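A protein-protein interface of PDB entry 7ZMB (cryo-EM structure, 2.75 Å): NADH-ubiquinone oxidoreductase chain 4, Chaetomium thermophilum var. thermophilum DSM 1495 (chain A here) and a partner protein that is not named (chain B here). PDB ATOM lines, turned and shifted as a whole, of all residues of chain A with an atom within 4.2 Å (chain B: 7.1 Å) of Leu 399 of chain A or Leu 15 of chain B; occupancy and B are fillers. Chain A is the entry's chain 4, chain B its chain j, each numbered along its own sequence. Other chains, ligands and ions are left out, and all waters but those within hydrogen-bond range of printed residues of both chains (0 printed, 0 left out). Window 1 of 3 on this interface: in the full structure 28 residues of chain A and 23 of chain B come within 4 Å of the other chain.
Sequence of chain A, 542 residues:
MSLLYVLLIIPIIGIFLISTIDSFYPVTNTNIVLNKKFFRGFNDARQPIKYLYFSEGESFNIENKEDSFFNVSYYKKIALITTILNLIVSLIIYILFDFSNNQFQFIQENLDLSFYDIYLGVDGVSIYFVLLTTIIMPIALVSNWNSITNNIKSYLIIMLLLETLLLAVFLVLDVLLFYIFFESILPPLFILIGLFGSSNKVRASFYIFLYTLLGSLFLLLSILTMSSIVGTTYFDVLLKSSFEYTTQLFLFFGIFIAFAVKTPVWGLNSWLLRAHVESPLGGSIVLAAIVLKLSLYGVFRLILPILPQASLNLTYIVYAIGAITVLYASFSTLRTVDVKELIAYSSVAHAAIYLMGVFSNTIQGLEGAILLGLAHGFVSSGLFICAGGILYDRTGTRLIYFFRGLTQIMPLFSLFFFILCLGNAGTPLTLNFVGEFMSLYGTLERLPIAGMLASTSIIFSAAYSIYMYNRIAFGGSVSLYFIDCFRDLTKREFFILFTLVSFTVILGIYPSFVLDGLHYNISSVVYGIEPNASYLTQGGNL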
ATOM      1  N   VAL A 337       1.404  -2.315  13.204  1.00  0.00           N
ATOM      2  CA  VAL A 337       1.035  -1.647  11.961  1.00  0.00           C
ATOM      3  C   VAL A 337      -0.177  -0.743  12.141  1.00  0.00           C
ATOM      4  O   VAL A 337      -0.239   0.338  11.560  1.00  0.00           O
ATOM      5  CB  VAL A 337       0.787  -2.699  10.860  1.00  0.00           C
ATOM      6  CG1 VAL A 337       0.301  -2.038   9.593  1.00  0.00           C
ATOM      7  CG2 VAL A 337       2.051  -3.488  10.598  1.00  0.00           C
ATOM      8  N   THR A 397      -8.683   4.807   7.593  1.00  0.00           N
ATOM      9  CA  THR A 397      -7.792   3.681   7.802  1.00  0.00           C
ATOM     10  C   THR A 397      -6.868   3.975   8.972  1.00  0.00           C
ATOM     11  O   THR A 397      -6.680   5.123   9.373  1.00  0.00           O
ATOM     12  CB  THR A 397      -6.959   3.363   6.549  1.00  0.00           C
ATOM     13  OG1 THR A 397      -6.036   2.305   6.837  1.00  0.00           O
ATOM     14  CG2 THR A 397      -6.184   4.583   6.084  1.00  0.00           C
ATOM     15  N   ARG A 398      -6.239   2.924   9.504  1.00  0.00           N
ATOM     16  CA  ARG A 398      -5.308   3.070  10.647  1.00  0.00           C
ATOM     17  C   ARG A 398      -4.023   2.319  10.322  1.00  0.00           C
ATOM     18  O   ARG A 398      -3.235   2.112  11.235  1.00  0.00           O
ATOM     19  CB  ARG A 398      -5.906   2.466  11.924  1.00  0.00           C
ATOM     20  CG  ARG A 398      -7.218   3.087  12.378  1.00  0.00           C
ATOM     21  CD  ARG A 398      -7.647   2.516  13.714  1.00  0.00           C
ATOM     22  NE  ARG A 398      -9.088   2.552  13.915  1.00  0.00           N
ATOM     23  CZ  ARG A 398      -9.754   3.571  14.444  1.00  0.00           C
ATOM     24  NH1 ARG A 398      -9.109   4.659  14.827  1.00  0.00           N
ATOM     25  NH2 ARG A 398     -11.065   3.501  14.582  1.00  0.00           N
ATOM     26  N   LEU A 399      -3.862   1.876   9.071  1.00  0.00           N
ATOM     27  CA  LEU A 399      -2.652   1.178   8.669  1.00  0.00           C
ATOM     28  C   LEU A 399      -1.549   2.192   8.406  1.00  0.00           C
ATOM     29  O   LEU A 399      -1.700   3.075   7.557  1.00  0.00           O
ATOM     30  CB  LEU A 399      -2.920   0.338   7.425  1.00  0.00           C
ATOM     31  CG  LEU A 399      -3.878  -0.834   7.593  1.00  0.00           C
ATOM     32  CD1 LEU A 399      -3.633  -1.866   6.511  1.00  0.00           C
ATOM     33  CD2 LEU A 399      -3.735  -1.443   8.976  1.00  0.00           C
ATOM     34  N   ILE A 400      -0.436   2.053   9.126  1.00  0.00           N
ATOM     35  CA  ILE A 400       0.674   2.985   8.995  1.00  0.00           C
ATOM     36  C   ILE A 400       1.306   2.933   7.607  1.00  0.00           C
ATOM     37  O   ILE A 400       2.025   3.860   7.225  1.00  0.00           O
ATOM     38  CB  ILE A 400       1.712   2.706  10.101  1.00  0.00           C
ATOM     39  CG1 ILE A 400       2.597   3.934  10.326  1.00  0.00           C
ATOM     40  CG2 ILE A 400       2.528   1.470   9.772  1.00  0.00           C
ATOM     41  CD1 ILE A 400       3.362   3.907  11.608  1.00  0.00           C
ATOM     42  N   TYR A 401       1.046   1.871   6.837  1.00  0.00           N
ATOM     43  CA  TYR A 401       1.518   1.790   5.458  1.00  0.00           C
ATOM     44  C   TYR A 401       1.057   2.962   4.616  1.00  0.00           C
ATOM     45  O   TYR A 401       1.747   3.340   3.664  1.00  0.00           O
ATOM     46  CB  TYR A 401       1.014   0.519   4.781  1.00  0.00           C
ATOM     47  CG  TYR A 401       1.283  -0.771   5.505  1.00  0.00           C
ATOM     48  CD1 TYR A 401       2.473  -0.978   6.177  1.00  0.00           C
ATOM     49  CD2 TYR A 401       0.349  -1.794   5.491  1.00  0.00           C
ATOM     50  CE1 TYR A 401       2.721  -2.167   6.828  1.00  0.00           C
ATOM     51  CE2 TYR A 401       0.591  -2.988   6.140  1.00  0.00           C
ATOM     52  CZ  TYR A 401       1.780  -3.167   6.801  1.00  0.00           C
ATOM     53  OH  TYR A 401       2.029  -4.349   7.451  1.00  0.00           O
ATOM     54  N   PHE A 402      -0.100   3.526   4.928  1.00  0.00           N
ATOM     55  CA  PHE A 402      -0.723   4.545   4.106  1.00  0.00           C
ATOM     56  C   PHE A 402      -0.319   5.956   4.494  1.00  0.00           C
ATOM     57  O   PHE A 402      -0.796   6.907   3.875  1.00  0.00           O
ATOM     58  CB  PHE A 402      -2.240   4.427   4.195  1.00  0.00           C
ATOM     59  CG  PHE A 402      -2.811   3.296   3.406  1.00  0.00           C
ATOM     60  CD1 PHE A 402      -2.780   3.314   2.032  1.00  0.00           C
ATOM     61  CD2 PHE A 402      -3.417   2.235   4.044  1.00  0.00           C
ATOM     62  CE1 PHE A 402      -3.324   2.285   1.304  1.00  0.00           C
ATOM     63  CE2 PHE A 402      -3.958   1.202   3.323  1.00  0.00           C
ATOM     64  CZ  PHE A 402      -3.915   1.226   1.950  1.00  0.00           C
ATOM     65  N   PHE A 403       0.511   6.117   5.517  1.00  0.00           N
ATOM     66  CA  PHE A 403       0.866   7.428   6.035  1.00  0.00           C
ATOM     67  C   PHE A 403       2.362   7.637   5.911  1.00  0.00           C
ATOM     68  O   PHE A 403       3.153   6.730   6.177  1.00  0.00           O
ATOM     69  CB  PHE A 403       0.440   7.599   7.486  1.00  0.00           C
ATOM     70  CG  PHE A 403      -1.021   7.395   7.715  1.00  0.00           C
ATOM     71  CD1 PHE A 403      -1.898   8.454   7.629  1.00  0.00           C
ATOM     72  CD2 PHE A 403      -1.517   6.143   8.016  1.00  0.00           C
ATOM     73  CE1 PHE A 403      -3.242   8.263   7.840  1.00  0.00           C
ATOM     74  CE2 PHE A 403      -2.858   5.948   8.223  1.00  0.00           C
ATOM     75  CZ  PHE A 403      -3.723   7.003   8.138  1.00  0.00           C
ATOM     76  N   TYR A 481      -0.723   7.380  -1.532  1.00  0.00           N
ATOM     77  CA  TYR A 481      -2.067   6.830  -1.521  1.00  0.00           C
ATOM     78  C   TYR A 481      -3.133   7.890  -1.254  1.00  0.00           C
ATOM     79  O   TYR A 481      -4.324   7.587  -1.363  1.00  0.00           O
ATOM     80  CB  TYR A 481      -2.171   5.712  -0.490  1.00  0.00           C
ATOM     81  CG  TYR A 481      -1.079   4.673  -0.569  1.00  0.00           C
ATOM     82  CD1 TYR A 481       0.126   4.852   0.086  1.00  0.00           C
ATOM     83  CD2 TYR A 481      -1.267   3.494  -1.272  1.00  0.00           C
ATOM     84  CE1 TYR A 481       1.117   3.905   0.025  1.00  0.00           C
ATOM     85  CE2 TYR A 481      -0.278   2.534  -1.333  1.00  0.00           C
ATOM     86  CZ  TYR A 481       0.913   2.749  -0.683  1.00  0.00           C
ATOM     87  OH  TYR A 481       1.903   1.803  -0.738  1.00  0.00           O
ATOM     88  N   ALA B  10      -6.149   6.046  -2.122  1.00  0.00           N
ATOM     89  CA  ALA B  10      -5.765   4.996  -3.065  1.00  0.00           C
ATOM     90  C   ALA B  10      -5.500   3.713  -2.283  1.00  0.00           C
ATOM     91  O   ALA B  10      -4.362   3.308  -2.042  1.00  0.00           O
ATOM     92  CB  ALA B  10      -4.549   5.410  -3.878  1.00  0.00           C
ATOM     93  N   MET B  11      -6.587   3.062  -1.885  1.00  0.00           N
ATOM     94  CA  MET B  11      -6.498   1.835  -1.112  1.00  0.00           C
ATOM     95  C   MET B  11      -5.824   0.745  -1.928  1.00  0.00           C
ATOM     96  O   MET B  11      -6.309   0.361  -2.997  1.00  0.00           O
ATOM     97  CB  MET B  11      -7.895   1.396  -0.682  1.00  0.00           C
ATOM     98  CG  MET B  11      -8.562   2.352   0.282  1.00  0.00           C
ATOM     99  SD  MET B  11      -7.647   2.539   1.821  1.00  0.00           S
ATOM    100  CE  MET B  11      -7.895   0.924   2.551  1.00  0.00           C
ATOM    101  N   ASP B  12      -4.711   0.242  -1.415  1.00  0.00           N
ATOM    102  CA  ASP B  12      -3.924  -0.753  -2.121  1.00  0.00           C
ATOM    103  C   ASP B  12      -4.374  -2.145  -1.707  1.00  0.00           C
ATOM    104  O   ASP B  12      -4.178  -2.520  -0.545  1.00  0.00           O
ATOM    105  CB  ASP B  12      -2.452  -0.578  -1.814  1.00  0.00           C
ATOM    106  CG  ASP B  12      -1.563  -1.368  -2.745  1.00  0.00           C
ATOM    107  OD1 ASP B  12      -2.081  -2.090  -3.613  1.00  0.00           O
ATOM    108  OD2 ASP B  12      -0.331  -1.260  -2.606  1.00  0.00           O
ATOM    109  N   PRO B  13      -4.934  -2.946  -2.611  1.00  0.00           N
ATOM    110  CA  PRO B  13      -5.399  -4.284  -2.210  1.00  0.00           C
ATOM    111  C   PRO B  13      -4.323  -5.123  -1.543  1.00  0.00           C
ATOM    112  O   PRO B  13      -4.626  -5.879  -0.613  1.00  0.00           O
ATOM    113  CB  PRO B  13      -5.856  -4.902  -3.539  1.00  0.00           C
ATOM    114  CG  PRO B  13      -6.186  -3.737  -4.405  1.00  0.00           C
ATOM    115  CD  PRO B  13      -5.227  -2.650  -4.022  1.00  0.00           C
ATOM    116  N   ALA B  14      -3.073  -5.012  -1.992  1.00  0.00           N
ATOM    117  CA  ALA B  14      -1.997  -5.729  -1.325  1.00  0.00           C
ATOM    118  C   ALA B  14      -1.829  -5.245   0.108  1.00  0.00           C
ATOM    119  O   ALA B  14      -1.655  -6.052   1.030  1.00  0.00           O
ATOM    120  CB  ALA B  14      -0.693  -5.564  -2.104  1.00  0.00           C
ATOM    121  N   LEU B  15      -1.871  -3.927   0.313  1.00  0.00           N
ATOM    122  CA  LEU B  15      -1.850  -3.383   1.664  1.00  0.00           C
ATOM    123  C   LEU B  15      -3.135  -3.719   2.401  1.00  0.00           C
ATOM    124  O   LEU B  15      -3.105  -4.051   3.591  1.00  0.00           O
ATOM    125  CB  LEU B  15      -1.645  -1.870   1.617  1.00  0.00           C
ATOM    126  CG  LEU B  15      -0.225  -1.306   1.610  1.00  0.00           C
ATOM    127  CD1 LEU B  15       0.591  -1.903   0.496  1.00  0.00           C
ATOM    128  CD2 LEU B  15      -0.289   0.195   1.474  1.00  0.00           C
ATOM    129  N   VAL B  16      -4.270  -3.641   1.708  1.00  0.00           N
ATOM    130  CA  VAL B  16      -5.548  -3.973   2.332  1.00  0.00           C
ATOM    131  C   VAL B  16      -5.565  -5.431   2.769  1.00  0.00           C
ATOM    132  O   VAL B  16      -6.002  -5.755   3.877  1.00  0.00           O
ATOM    133  CB  VAL B  16      -6.713  -3.651   1.380  1.00  0.00           C
ATOM    134  CG1 VAL B  16      -8.034  -4.097   1.987  1.00  0.00           C
ATOM    135  CG2 VAL B  16      -6.758  -2.168   1.093  1.00  0.00           C
ATOM    136  N   ARG B  17      -5.082  -6.334   1.916  1.00  0.00           N
ATOM    137  CA  ARG B  17      -5.101  -7.746   2.276  1.00  0.00           C
ATOM    138  C   ARG B  17      -4.039  -8.088   3.309  1.00  0.00           C
ATOM    139  O   ARG B  17      -4.238  -9.011   4.103  1.00  0.00           O
ATOM    140  CB  ARG B  17      -4.948  -8.621   1.029  1.00  0.00           C
ATOM    141  CG  ARG B  17      -3.548  -8.721   0.466  1.00  0.00           C
ATOM    142  CD  ARG B  17      -3.536  -9.568  -0.791  1.00  0.00           C
ATOM    143  NE  ARG B  17      -4.380  -8.994  -1.835  1.00  0.00           N
ATOM    144  CZ  ARG B  17      -4.698  -9.619  -2.963  1.00  0.00           C
ATOM    145  NH1 ARG B  17      -5.473  -9.022  -3.858  1.00  0.00           N
ATOM    146  NH2 ARG B  17      -4.242 -10.841  -3.197  1.00  0.00           N
ATOM    147  N   LEU B  18      -2.923  -7.363   3.326  1.00  0.00           N
ATOM    148  CA  LEU B  18      -1.926  -7.576   4.371  1.00  0.00           C
ATOM    149  C   LEU B  18      -2.478  -7.223   5.746  1.00  0.00           C
ATOM    150  O   LEU B  18      -2.168  -7.892   6.737  1.00  0.00           O
ATOM    151  CB  LEU B  18      -0.667  -6.772   4.063  1.00  0.00           C
ATOM    152  CG  LEU B  18       0.511  -6.918   5.021  1.00  0.00           C
ATOM    153  CD1 LEU B  18       1.018  -8.323   5.046  1.00  0.00           C
ATOM    154  CD2 LEU B  18       1.605  -5.994   4.567  1.00  0.00           C
ATOM    155  N   GLY B  19      -3.293  -6.171   5.829  1.00  0.00           N
ATOM    156  CA  GLY B  19      -3.961  -5.853   7.077  1.00  0.00           C
ATOM    157  C   GLY B  19      -4.950  -6.915   7.510  1.00  0.00           C
ATOM    158  O   GLY B  19      -5.114  -7.161   8.708  1.00  0.00           O
ATOM    159  N   SER B  20      -5.627  -7.551   6.553  1.00  0.00           N
ATOM    160  CA  SER B  20      -6.565  -8.614   6.898  1.00  0.00           C
ATOM    161  C   SER B  20      -5.857  -9.792   7.546  1.00  0.00           C
ATOM    162  O   SER B  20      -6.344 -10.347   8.535  1.00  0.00           O
ATOM    163  CB  SER B  20      -7.321  -9.073   5.655  1.00  0.00           C
ATOM    164  OG  SER B  20      -8.209 -10.127   5.971  1.00  0.00           O
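O of Tyr 481 of chain A sits at hydrogen-bond distance from N of Ala 10 of chain B (2.5 Å).
Val 337 of chain A touches none of the printed residues of chain B. Leu 399 of chain A touches one residue of chain B. Of the printed residues of chain B, Tyr 401 of chain A touches Leu 15 and Leu 18. Printed residues of chain A within 4 Å of Ala 10 of chain B: Phe 402 (3.6 Å) and Tyr 481 (2.5 Å). Printed residues of chain A within 4 Å of Met 11 of chain B: Phe 402. Printed residues of chain A within 4 Å of Asp 12 of chain B: Phe 402 and Tyr 481. Pro 13 of chain B touches none of the printed residues of chain A. Of chain A, only Leu 399, Tyr 401, Phe 402 and Tyr 481 come within 4 Å of Leu 15 of chain B. The nearest printed residue of chain A that does not touch Leu 15 of chain B is Ile 400 of chain A (6.9 Å).
N of Leu 399 of chain A is in hydrogen-bond range of OG1 of Thr 397 of chain A (3.1 Å). The backbone NH (N) of Ala 14 of chain B lies close to the side-chain carboxylate (OD1) of Asp 12 of chain B, at 3.5 Å.
Among the printed residues, pairs that only touch across the chains: Tyr 401 of chain A with Leu 18 of chain B (3.3 Å), Tyr 481 of chain A with Leu 15 of chain B (3.5 Å), Tyr 401 of chain A with Leu 15 of chain B (3.6 Å), Phe 402 of chain A with Asp 12 of chain B (3.6 Å), Phe 402 of chain A with Ala 10 of chain B (3.6 Å), Leu 399 of chain A with Leu 15 of chain B (3.7 Å), Phe 402 of chain A with Leu 15 of chain B (3.7 Å), Tyr 481 of chain A with Asp 12 of chain B (3.8 Å) and Phe 402 of chain A with Met 11 of chain B (3.96 Å).
Hydrophobic or aromatic side chains of chain B that line the printed part of chain A: Ala 10, Met 11, Leu 15 and Leu 18. Of the 9 printed residues of chain A, 4 touch a printed residue of chain B. Among the printed residues, no Asp or Glu carboxylate lies within 4 Å of a Lys or Arg side-chain nitrogen of the other chain.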
